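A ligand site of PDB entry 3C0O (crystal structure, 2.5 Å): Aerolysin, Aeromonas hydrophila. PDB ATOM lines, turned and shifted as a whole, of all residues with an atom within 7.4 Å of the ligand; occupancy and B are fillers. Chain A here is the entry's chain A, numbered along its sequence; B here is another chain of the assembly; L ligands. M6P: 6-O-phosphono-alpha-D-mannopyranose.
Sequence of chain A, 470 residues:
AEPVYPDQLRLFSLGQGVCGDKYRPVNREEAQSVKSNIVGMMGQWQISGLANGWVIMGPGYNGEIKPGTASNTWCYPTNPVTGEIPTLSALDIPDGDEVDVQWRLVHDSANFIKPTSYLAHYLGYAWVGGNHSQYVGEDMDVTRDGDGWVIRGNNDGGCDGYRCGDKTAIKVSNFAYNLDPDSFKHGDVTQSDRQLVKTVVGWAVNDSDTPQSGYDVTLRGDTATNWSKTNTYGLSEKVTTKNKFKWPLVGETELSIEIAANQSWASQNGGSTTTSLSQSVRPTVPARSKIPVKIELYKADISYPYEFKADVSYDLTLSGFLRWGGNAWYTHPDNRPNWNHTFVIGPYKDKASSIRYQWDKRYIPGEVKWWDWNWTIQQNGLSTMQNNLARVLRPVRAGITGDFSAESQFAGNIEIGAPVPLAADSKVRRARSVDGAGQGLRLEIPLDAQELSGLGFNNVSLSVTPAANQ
The guanidinium group (NH2) of Arg 163 is in hydrogen-bond range of the backbone carbonyl oxygen (O) of Arg 336, at 3.2 Å. O of Tyr 162 is in hydrogen-bond range of NE1 of Trp 127 (3.0 Å). The backbone carbonyl oxygen of Arg 163 lies within hydrogen-bond range of the indole nitrogen of Trp 127 (3.3 Å). The backbone NH (N) of Thr 168 is in hydrogen-bond range of the backbone carbonyl oxygen (O) of Trp 127, 3.1 Å away. The backbone carbonyl oxygen of Gly 124 is in hydrogen-bond range of the backbone NH of Arg 323 (2.7 Å). The backbone carbonyl oxygen (O) of Phe 321 sits at hydrogen-bond distance from the backbone NH (N) of Ala 126, at 3.1 Å. O of Ala 126 is in hydrogen-bond range of OG1 of Thr 168 (2.6 Å).
Ala 126 touches the ligand (CA to O1, 3.7 Å). Phe 321 touches the ligand (CE1 to O2P, 3.98 Å). Of the 25 residues printed, 6 come within 4 Å of the ligand.
The backbone NH of Trp 324 is in hydrogen-bond range of an oxygen (O2P) of the ligand, at 2.6 Å. The backbone carbonyl oxygen (O) of Trp 324 lies close to an oxygen (O3P) of the ligand, at 2.6 Å. The guanidinium group (NE) of Arg 336 is in salt-bridge range of an oxygen (O2P) of the ligand, at 2.8 Å. N of Trp 127 sits at hydrogen-bond distance from O1 of the ligand (2.9 Å). The guanidinium group of Arg 323 is in salt-bridge range of an oxygen (O3P) of the ligand, at 3.6 Å.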
ATOM      1  N   HIS A 121      20.399  18.427 -22.968  1.00  0.00           N
ATOM      2  CA  HIS A 121      21.237  18.093 -24.108  1.00  0.00           C
ATOM      3  C   HIS A 121      22.723  17.945 -23.620  1.00  0.00           C
ATOM      4  O   HIS A 121      23.452  17.030 -24.075  1.00  0.00           O
ATOM      5  CB  HIS A 121      21.093  19.204 -25.180  1.00  0.00           C
ATOM      6  CG  HIS A 121      22.175  19.197 -26.239  1.00  0.00           C
ATOM      7  ND1 HIS A 121      22.226  18.253 -27.252  1.00  0.00           N
ATOM      8  CD2 HIS A 121      23.212  20.051 -26.469  1.00  0.00           C
ATOM      9  CE1 HIS A 121      23.281  18.493 -28.026  1.00  0.00           C
ATOM     10  NE2 HIS A 121      23.898  19.574 -27.567  1.00  0.00           N
ATOM     11  N   GLY A 124      23.391  14.579 -22.268  1.00  0.00           N
ATOM     12  CA  GLY A 124      23.265  13.415 -23.136  1.00  0.00           C
ATOM     13  C   GLY A 124      21.861  12.865 -23.474  1.00  0.00           C
ATOM     14  O   GLY A 124      21.746  11.766 -24.112  1.00  0.00           O
ATOM     15  N   TYR A 125      20.796  13.574 -23.071  1.00  0.00           N
ATOM     16  CA  TYR A 125      19.474  13.136 -23.397  1.00  0.00           C
ATOM     17  C   TYR A 125      19.276  13.343 -24.887  1.00  0.00           C
ATOM     18  O   TYR A 125      19.823  14.304 -25.461  1.00  0.00           O
ATOM     19  CB  TYR A 125      18.445  13.940 -22.625  1.00  0.00           C
ATOM     20  CG  TYR A 125      18.271  13.486 -21.217  1.00  0.00           C
ATOM     21  CD1 TYR A 125      19.092  14.005 -20.167  1.00  0.00           C
ATOM     22  CD2 TYR A 125      17.311  12.545 -20.871  1.00  0.00           C
ATOM     23  CE1 TYR A 125      18.961  13.618 -18.861  1.00  0.00           C
ATOM     24  CE2 TYR A 125      17.179  12.137 -19.519  1.00  0.00           C
ATOM     25  CZ  TYR A 125      18.003  12.681 -18.540  1.00  0.00           C
ATOM     26  OH  TYR A 125      17.823  12.296 -17.221  1.00  0.00           O
ATOM     27  N   ALA A 126      18.538  12.450 -25.532  1.00  0.00           N
ATOM     28  CA  ALA A 126      18.486  12.452 -26.994  1.00  0.00           C
ATOM     29  C   ALA A 126      17.362  13.365 -27.416  1.00  0.00           C
ATOM     30  O   ALA A 126      16.373  13.442 -26.712  1.00  0.00           O
ATOM     31  CB  ALA A 126      18.211  11.009 -27.514  1.00  0.00           C
ATOM     32  N   TRP A 127      17.489  14.055 -28.547  1.00  0.00           N
ATOM     33  CA  TRP A 127      16.330  14.735 -29.140  1.00  0.00           C
ATOM     34  C   TRP A 127      15.636  15.721 -28.192  1.00  0.00           C
ATOM     35  O   TRP A 127      14.453  15.630 -27.850  1.00  0.00           O
ATOM     36  CB  TRP A 127      15.322  13.714 -29.663  1.00  0.00           C
ATOM     37  CG  TRP A 127      15.924  12.717 -30.624  1.00  0.00           C
ATOM     38  CD1 TRP A 127      15.991  11.343 -30.464  1.00  0.00           C
ATOM     39  CD2 TRP A 127      16.517  13.005 -31.900  1.00  0.00           C
ATOM     40  NE1 TRP A 127      16.594  10.771 -31.541  1.00  0.00           N
ATOM     41  CE2 TRP A 127      16.931  11.761 -32.441  1.00  0.00           C
ATOM     42  CE3 TRP A 127      16.709  14.161 -32.652  1.00  0.00           C
ATOM     43  CZ2 TRP A 127      17.541  11.669 -33.691  1.00  0.00           C
ATOM     44  CZ3 TRP A 127      17.327  14.083 -33.838  1.00  0.00           C
ATOM     45  CH2 TRP A 127      17.749  12.833 -34.374  1.00  0.00           C
ATOM     46  N   VAL A 128      16.397  16.701 -27.767  1.00  0.00           N
ATOM     47  CA  VAL A 128      15.779  17.749 -26.989  1.00  0.00           C
ATOM     48  C   VAL A 128      15.385  18.892 -27.950  1.00  0.00           C
ATOM     49  O   VAL A 128      16.119  19.888 -28.104  1.00  0.00           O
ATOM     50  CB  VAL A 128      16.705  18.195 -25.824  1.00  0.00           C
ATOM     51  CG1 VAL A 128      15.988  19.166 -24.966  1.00  0.00           C
ATOM     52  CG2 VAL A 128      17.130  17.000 -25.014  1.00  0.00           C
ATOM     53  N   ASP A 160      13.585  12.539 -39.166  1.00  0.00           N
ATOM     54  CA  ASP A 160      14.788  11.794 -39.561  1.00  0.00           C
ATOM     55  C   ASP A 160      15.721  11.811 -38.353  1.00  0.00           C
ATOM     56  O   ASP A 160      15.648  12.715 -37.506  1.00  0.00           O
ATOM     57  CB  ASP A 160      15.489  12.488 -40.749  1.00  0.00           C
ATOM     58  CG  ASP A 160      14.874  12.154 -42.116  1.00  0.00           C
ATOM     59  OD1 ASP A 160      13.699  12.550 -42.373  1.00  0.00           O
ATOM     60  OD2 ASP A 160      15.595  11.514 -42.930  1.00  0.00           O
ATOM     61  N   GLY A 161      16.632  10.842 -38.340  1.00  0.00           N
ATOM     62  CA  GLY A 161      17.514  10.602 -37.205  1.00  0.00           C
ATOM     63  C   GLY A 161      17.162   9.284 -36.543  1.00  0.00           C
ATOM     64  O   GLY A 161      16.008   8.843 -36.531  1.00  0.00           O
ATOM     65  N   TYR A 162      18.163   8.638 -35.976  1.00  0.00           N
ATOM     66  CA  TYR A 162      17.941   7.367 -35.286  1.00  0.00           C
ATOM     67  C   TYR A 162      17.020   7.509 -34.049  1.00  0.00           C
ATOM     68  O   TYR A 162      17.278   8.314 -33.174  1.00  0.00           O
ATOM     69  CB  TYR A 162      19.290   6.728 -34.897  1.00  0.00           C
ATOM     70  CG  TYR A 162      19.117   5.451 -34.088  1.00  0.00           C
ATOM     71  CD1 TYR A 162      18.706   4.253 -34.696  1.00  0.00           C
ATOM     72  CD2 TYR A 162      19.313   5.457 -32.719  1.00  0.00           C
ATOM     73  CE1 TYR A 162      18.507   3.094 -33.937  1.00  0.00           C
ATOM     74  CE2 TYR A 162      19.137   4.343 -31.980  1.00  0.00           C
ATOM     75  CZ  TYR A 162      18.730   3.173 -32.575  1.00  0.00           C
ATOM     76  OH  TYR A 162      18.562   2.095 -31.764  1.00  0.00           O
ATOM     77  N   ARG A 163      15.925   6.770 -34.005  1.00  0.00           N
ATOM     78  CA  ARG A 163      15.049   6.835 -32.823  1.00  0.00           C
ATOM     79  C   ARG A 163      14.489   8.241 -32.578  1.00  0.00           C
ATOM     80  O   ARG A 163      14.096   8.584 -31.468  1.00  0.00           O
ATOM     81  CB  ARG A 163      15.852   6.401 -31.628  1.00  0.00           C
ATOM     82  CG  ARG A 163      15.037   6.043 -30.412  1.00  0.00           C
ATOM     83  CD  ARG A 163      14.999   4.513 -30.242  1.00  0.00           C
ATOM     84  NE  ARG A 163      15.949   4.014 -29.241  1.00  0.00           N
ATOM     85  CZ  ARG A 163      15.744   4.003 -27.916  1.00  0.00           C
ATOM     86  NH1 ARG A 163      14.658   4.513 -27.379  1.00  0.00           N
ATOM     87  NH2 ARG A 163      16.686   3.515 -27.105  1.00  0.00           N
ATOM     88  N   CYS A 164      14.385   9.059 -33.631  1.00  0.00           N
ATOM     89  CA  CYS A 164      14.016  10.476 -33.479  1.00  0.00           C
ATOM     90  C   CYS A 164      12.632  10.755 -32.916  1.00  0.00           C
ATOM     91  O   CYS A 164      12.398  11.852 -32.394  1.00  0.00           O
ATOM     92  CB  CYS A 164      14.189  11.229 -34.779  1.00  0.00           C
ATOM     93  SG  CYS A 164      13.116  10.678 -36.207  1.00  0.00           S
ATOM     94  N   ASP A 166      11.657   9.500 -30.181  1.00  0.00           N
ATOM     95  CA  ASP A 166      11.668   9.408 -28.716  1.00  0.00           C
ATOM     96  C   ASP A 166      12.193  10.701 -28.077  1.00  0.00           C
ATOM     97  O   ASP A 166      13.359  10.814 -27.717  1.00  0.00           O
ATOM     98  CB  ASP A 166      12.477   8.202 -28.262  1.00  0.00           C
ATOM     99  CG  ASP A 166      11.862   6.868 -28.694  1.00  0.00           C
ATOM    100  OD1 ASP A 166      10.603   6.765 -28.861  1.00  0.00           O
ATOM    101  OD2 ASP A 166      12.664   5.914 -28.860  1.00  0.00           O
ATOM    102  N   THR A 168      12.945  13.882 -25.730  1.00  0.00           N
ATOM    103  CA  THR A 168      13.160  14.053 -24.305  1.00  0.00           C
ATOM    104  C   THR A 168      12.107  15.021 -23.807  1.00  0.00           C
ATOM    105  O   THR A 168      11.728  15.973 -24.523  1.00  0.00           O
ATOM    106  CB  THR A 168      14.550  14.645 -23.979  1.00  0.00           C
ATOM    107  OG1 THR A 168      15.545  13.659 -24.289  1.00  0.00           O
ATOM    108  CG2 THR A 168      14.678  14.999 -22.540  1.00  0.00           C
ATOM    109  N   PHE A 321      16.158   9.036 -23.496  1.00  0.00           N
ATOM    110  CA  PHE A 321      17.208   8.034 -23.445  1.00  0.00           C
ATOM    111  C   PHE A 321      18.602   8.680 -23.553  1.00  0.00           C
ATOM    112  O   PHE A 321      18.733   9.731 -24.122  1.00  0.00           O
ATOM    113  CB  PHE A 321      16.967   6.929 -24.457  1.00  0.00           C
ATOM    114  CG  PHE A 321      17.262   7.335 -25.901  1.00  0.00           C
ATOM    115  CD1 PHE A 321      18.525   7.220 -26.418  1.00  0.00           C
ATOM    116  CD2 PHE A 321      16.245   7.718 -26.754  1.00  0.00           C
ATOM    117  CE1 PHE A 321      18.771   7.538 -27.784  1.00  0.00           C
ATOM    118  CE2 PHE A 321      16.493   8.078 -28.106  1.00  0.00           C
ATOM    119  CZ  PHE A 321      17.754   7.988 -28.602  1.00  0.00           C
ATOM    120  N   LEU A 322      19.620   8.067 -22.988  1.00  0.00           N
ATOM    121  CA  LEU A 322      20.943   8.662 -22.997  1.00  0.00           C
ATOM    122  C   LEU A 322      21.654   8.255 -24.240  1.00  0.00           C
ATOM    123  O   LEU A 322      21.666   7.075 -24.571  1.00  0.00           O
ATOM    124  CB  LEU A 322      21.740   8.166 -21.787  1.00  0.00           C
ATOM    125  CG  LEU A 322      20.979   8.640 -20.525  1.00  0.00           C
ATOM    126  CD1 LEU A 322      21.650   8.301 -19.222  1.00  0.00           C
ATOM    127  CD2 LEU A 322      20.701  10.132 -20.608  1.00  0.00           C
ATOM    128  N   ARG A 323      22.247   9.202 -24.954  1.00  0.00           N
ATOM    129  CA  ARG A 323      22.872   8.863 -26.192  1.00  0.00           C
ATOM    130  C   ARG A 323      24.054   7.911 -26.082  1.00  0.00           C
ATOM    131  O   ARG A 323      24.785   7.929 -25.096  1.00  0.00           O
ATOM    132  CB  ARG A 323      23.356  10.107 -26.901  1.00  0.00           C
ATOM    133  CG  ARG A 323      22.287  11.165 -27.123  1.00  0.00           C
ATOM    134  CD  ARG A 323      22.917  12.379 -27.802  1.00  0.00           C
ATOM    135  NE  ARG A 323      23.745  11.983 -28.944  1.00  0.00           N
ATOM    136  CZ  ARG A 323      24.702  12.746 -29.483  1.00  0.00           C
ATOM    137  NH1 ARG A 323      24.979  13.938 -28.989  1.00  0.00           N
ATOM    138  NH2 ARG A 323      25.400  12.291 -30.510  1.00  0.00           N
ATOM    139  N   TRP A 324      24.198   7.071 -27.118  1.00  0.00           N
ATOM    140  CA  TRP A 324      25.343   6.177 -27.221  1.00  0.00           C
ATOM    141  C   TRP A 324      26.512   7.018 -27.666  1.00  0.00           C
ATOM    142  O   TRP A 324      26.392   7.782 -28.617  1.00  0.00           O
ATOM    143  CB  TRP A 324      25.146   5.073 -28.263  1.00  0.00           C
ATOM    144  CG  TRP A 324      26.396   4.339 -28.562  1.00  0.00           C
ATOM    145  CD1 TRP A 324      26.830   3.193 -27.930  1.00  0.00           C
ATOM    146  CD2 TRP A 324      27.387   4.645 -29.542  1.00  0.00           C
ATOM    147  NE1 TRP A 324      28.033   2.793 -28.441  1.00  0.00           N
ATOM    148  CE2 TRP A 324      28.413   3.672 -29.421  1.00  0.00           C
ATOM    149  CE3 TRP A 324      27.532   5.662 -30.525  1.00  0.00           C
ATOM    150  CZ2 TRP A 324      29.570   3.689 -30.223  1.00  0.00           C
ATOM    151  CZ3 TRP A 324      28.670   5.681 -31.316  1.00  0.00           C
ATOM    152  CH2 TRP A 324      29.686   4.698 -31.140  1.00  0.00           C
ATOM    153  N   GLY A 325      27.662   6.928 -27.024  1.00  0.00           N
ATOM    154  CA  GLY A 325      28.794   7.686 -27.460  1.00  0.00           C
ATOM    155  C   GLY A 325      28.576   9.152 -27.153  1.00  0.00           C
ATOM    156  O   GLY A 325      28.736  10.011 -28.027  1.00  0.00           O
ATOM    157  N   GLY A 326      28.221   9.420 -25.915  1.00  0.00           N
ATOM    158  CA  GLY A 326      28.035  10.770 -25.566  1.00  0.00           C
ATOM    159  C   GLY A 326      27.010  11.046 -24.506  1.00  0.00           C
ATOM    160  O   GLY A 326      26.022  11.692 -24.795  1.00  0.00           O
ATOM    161  N   ASN A 335      23.975   1.833 -23.977  1.00  0.00           N
ATOM    162  CA  ASN A 335      22.882   1.071 -24.553  1.00  0.00           C
ATOM    163  C   ASN A 335      21.600   1.865 -24.637  1.00  0.00           C
ATOM    164  O   ASN A 335      20.510   1.277 -24.726  1.00  0.00           O
ATOM    165  CB  ASN A 335      22.664  -0.235 -23.765  1.00  0.00           C
ATOM    166  CG  ASN A 335      22.468  -0.023 -22.292  1.00  0.00           C
ATOM    167  OD1 ASN A 335      22.936   0.971 -21.757  1.00  0.00           O
ATOM    168  ND2 ASN A 335      21.784  -0.961 -21.637  1.00  0.00           N
ATOM    169  N   ARG A 336      21.680   3.191 -24.637  1.00  0.00           N
ATOM    170  CA  ARG A 336      20.528   3.998 -24.916  1.00  0.00           C
ATOM    171  C   ARG A 336      19.417   3.608 -23.995  1.00  0.00           C
ATOM    172  O   ARG A 336      18.282   3.447 -24.386  1.00  0.00           O
ATOM    173  CB  ARG A 336      20.119   3.744 -26.368  1.00  0.00           C
ATOM    174  CG  ARG A 336      21.189   4.154 -27.397  1.00  0.00           C
ATOM    175  CD  ARG A 336      20.589   4.331 -28.786  1.00  0.00           C
ATOM    176  NE  ARG A 336      21.625   4.713 -29.718  1.00  0.00           N
ATOM    177  CZ  ARG A 336      22.371   3.826 -30.404  1.00  0.00           C
ATOM    178  NH1 ARG A 336      22.191   2.487 -30.263  1.00  0.00           N
ATOM    179  NH2 ARG A 336      23.294   4.280 -31.245  1.00  0.00           N
ATOM    180  N   PRO B 286      30.619  15.209 -37.314  1.00  0.00           N
ATOM    181  CA  PRO B 286      30.737  13.867 -37.878  1.00  0.00           C
ATOM    182  C   PRO B 286      31.423  13.807 -39.243  1.00  0.00           C
ATOM    183  O   PRO B 286      31.572  14.827 -39.928  1.00  0.00           O
ATOM    184  CB  PRO B 286      29.270  13.404 -37.946  1.00  0.00           C
ATOM    185  CG  PRO B 286      28.635  14.078 -36.768  1.00  0.00           C
ATOM    186  CD  PRO B 286      29.311  15.419 -36.657  1.00  0.00           C
ATOM    187  N   GLY B 417      23.269  22.905 -34.694  1.00  0.00           N
ATOM    188  CA  GLY B 417      22.227  21.983 -35.093  1.00  0.00           C
ATOM    189  C   GLY B 417      22.692  20.546 -35.266  1.00  0.00           C
ATOM    190  O   GLY B 417      23.856  20.188 -35.032  1.00  0.00           O
ATOM    191  N   ALA B 418      21.747  19.715 -35.635  1.00  0.00           N
ATOM    192  CA  ALA B 418      22.002  18.375 -36.098  1.00  0.00           C
ATOM    193  C   ALA B 418      22.858  18.362 -37.373  1.00  0.00           C
ATOM    194  O   ALA B 418      22.481  18.959 -38.430  1.00  0.00           O
ATOM    195  CB  ALA B 418      20.663  17.656 -36.329  1.00  0.00           C
ATOM    196  N   PRO B 419      24.012  17.670 -37.283  1.00  0.00           N
ATOM    197  CA  PRO B 419      24.940  17.390 -38.359  1.00  0.00           C
ATOM    198  C   PRO B 419      24.252  16.644 -39.504  1.00  0.00           C
ATOM    199  O   PRO B 419      23.564  15.656 -39.283  1.00  0.00           O
ATOM    200  CB  PRO B 419      25.961  16.448 -37.683  1.00  0.00           C
ATOM    201  CG  PRO B 419      25.237  15.859 -36.546  1.00  0.00           C
ATOM    202  CD  PRO B 419      24.429  17.019 -36.038  1.00  0.00           C
HETATM  203  C1  M6P L   1      20.992  13.073 -30.605  1.00  0.00           C
HETATM  204  C2  M6P L   1      21.554  13.633 -31.899  1.00  0.00           C
HETATM  205  C3  M6P L   1      21.438  12.709 -33.111  1.00  0.00           C
HETATM  206  C4  M6P L   1      21.804  11.314 -32.696  1.00  0.00           C
HETATM  207  C5  M6P L   1      20.771  10.859 -31.705  1.00  0.00           C
HETATM  208  C6  M6P L   1      21.001   9.416 -31.312  1.00  0.00           C
HETATM  209  O1  M6P L   1      19.696  13.569 -30.301  1.00  0.00           O
HETATM  210  O2  M6P L   1      22.928  13.881 -31.644  1.00  0.00           O
HETATM  211  O3  M6P L   1      22.297  13.130 -34.190  1.00  0.00           O
HETATM  212  O4  M6P L   1      21.540  10.553 -33.843  1.00  0.00           O
HETATM  213  O5  M6P L   1      20.925  11.653 -30.544  1.00  0.00           O
HETATM  214  O6  M6P L   1      22.170   9.380 -30.502  1.00  0.00           O
HETATM  215  P   M6P L   1      23.089   8.059 -30.260  1.00  0.00           P
HETATM  216  O1P M6P L   1      23.074   7.335 -31.645  1.00  0.00           O
HETATM  217  O2P M6P L   1      22.507   7.274 -29.123  1.00  0.00           O
HETATM  218  O3P M6P L   1      24.473   8.670 -30.081  1.00  0.00           O
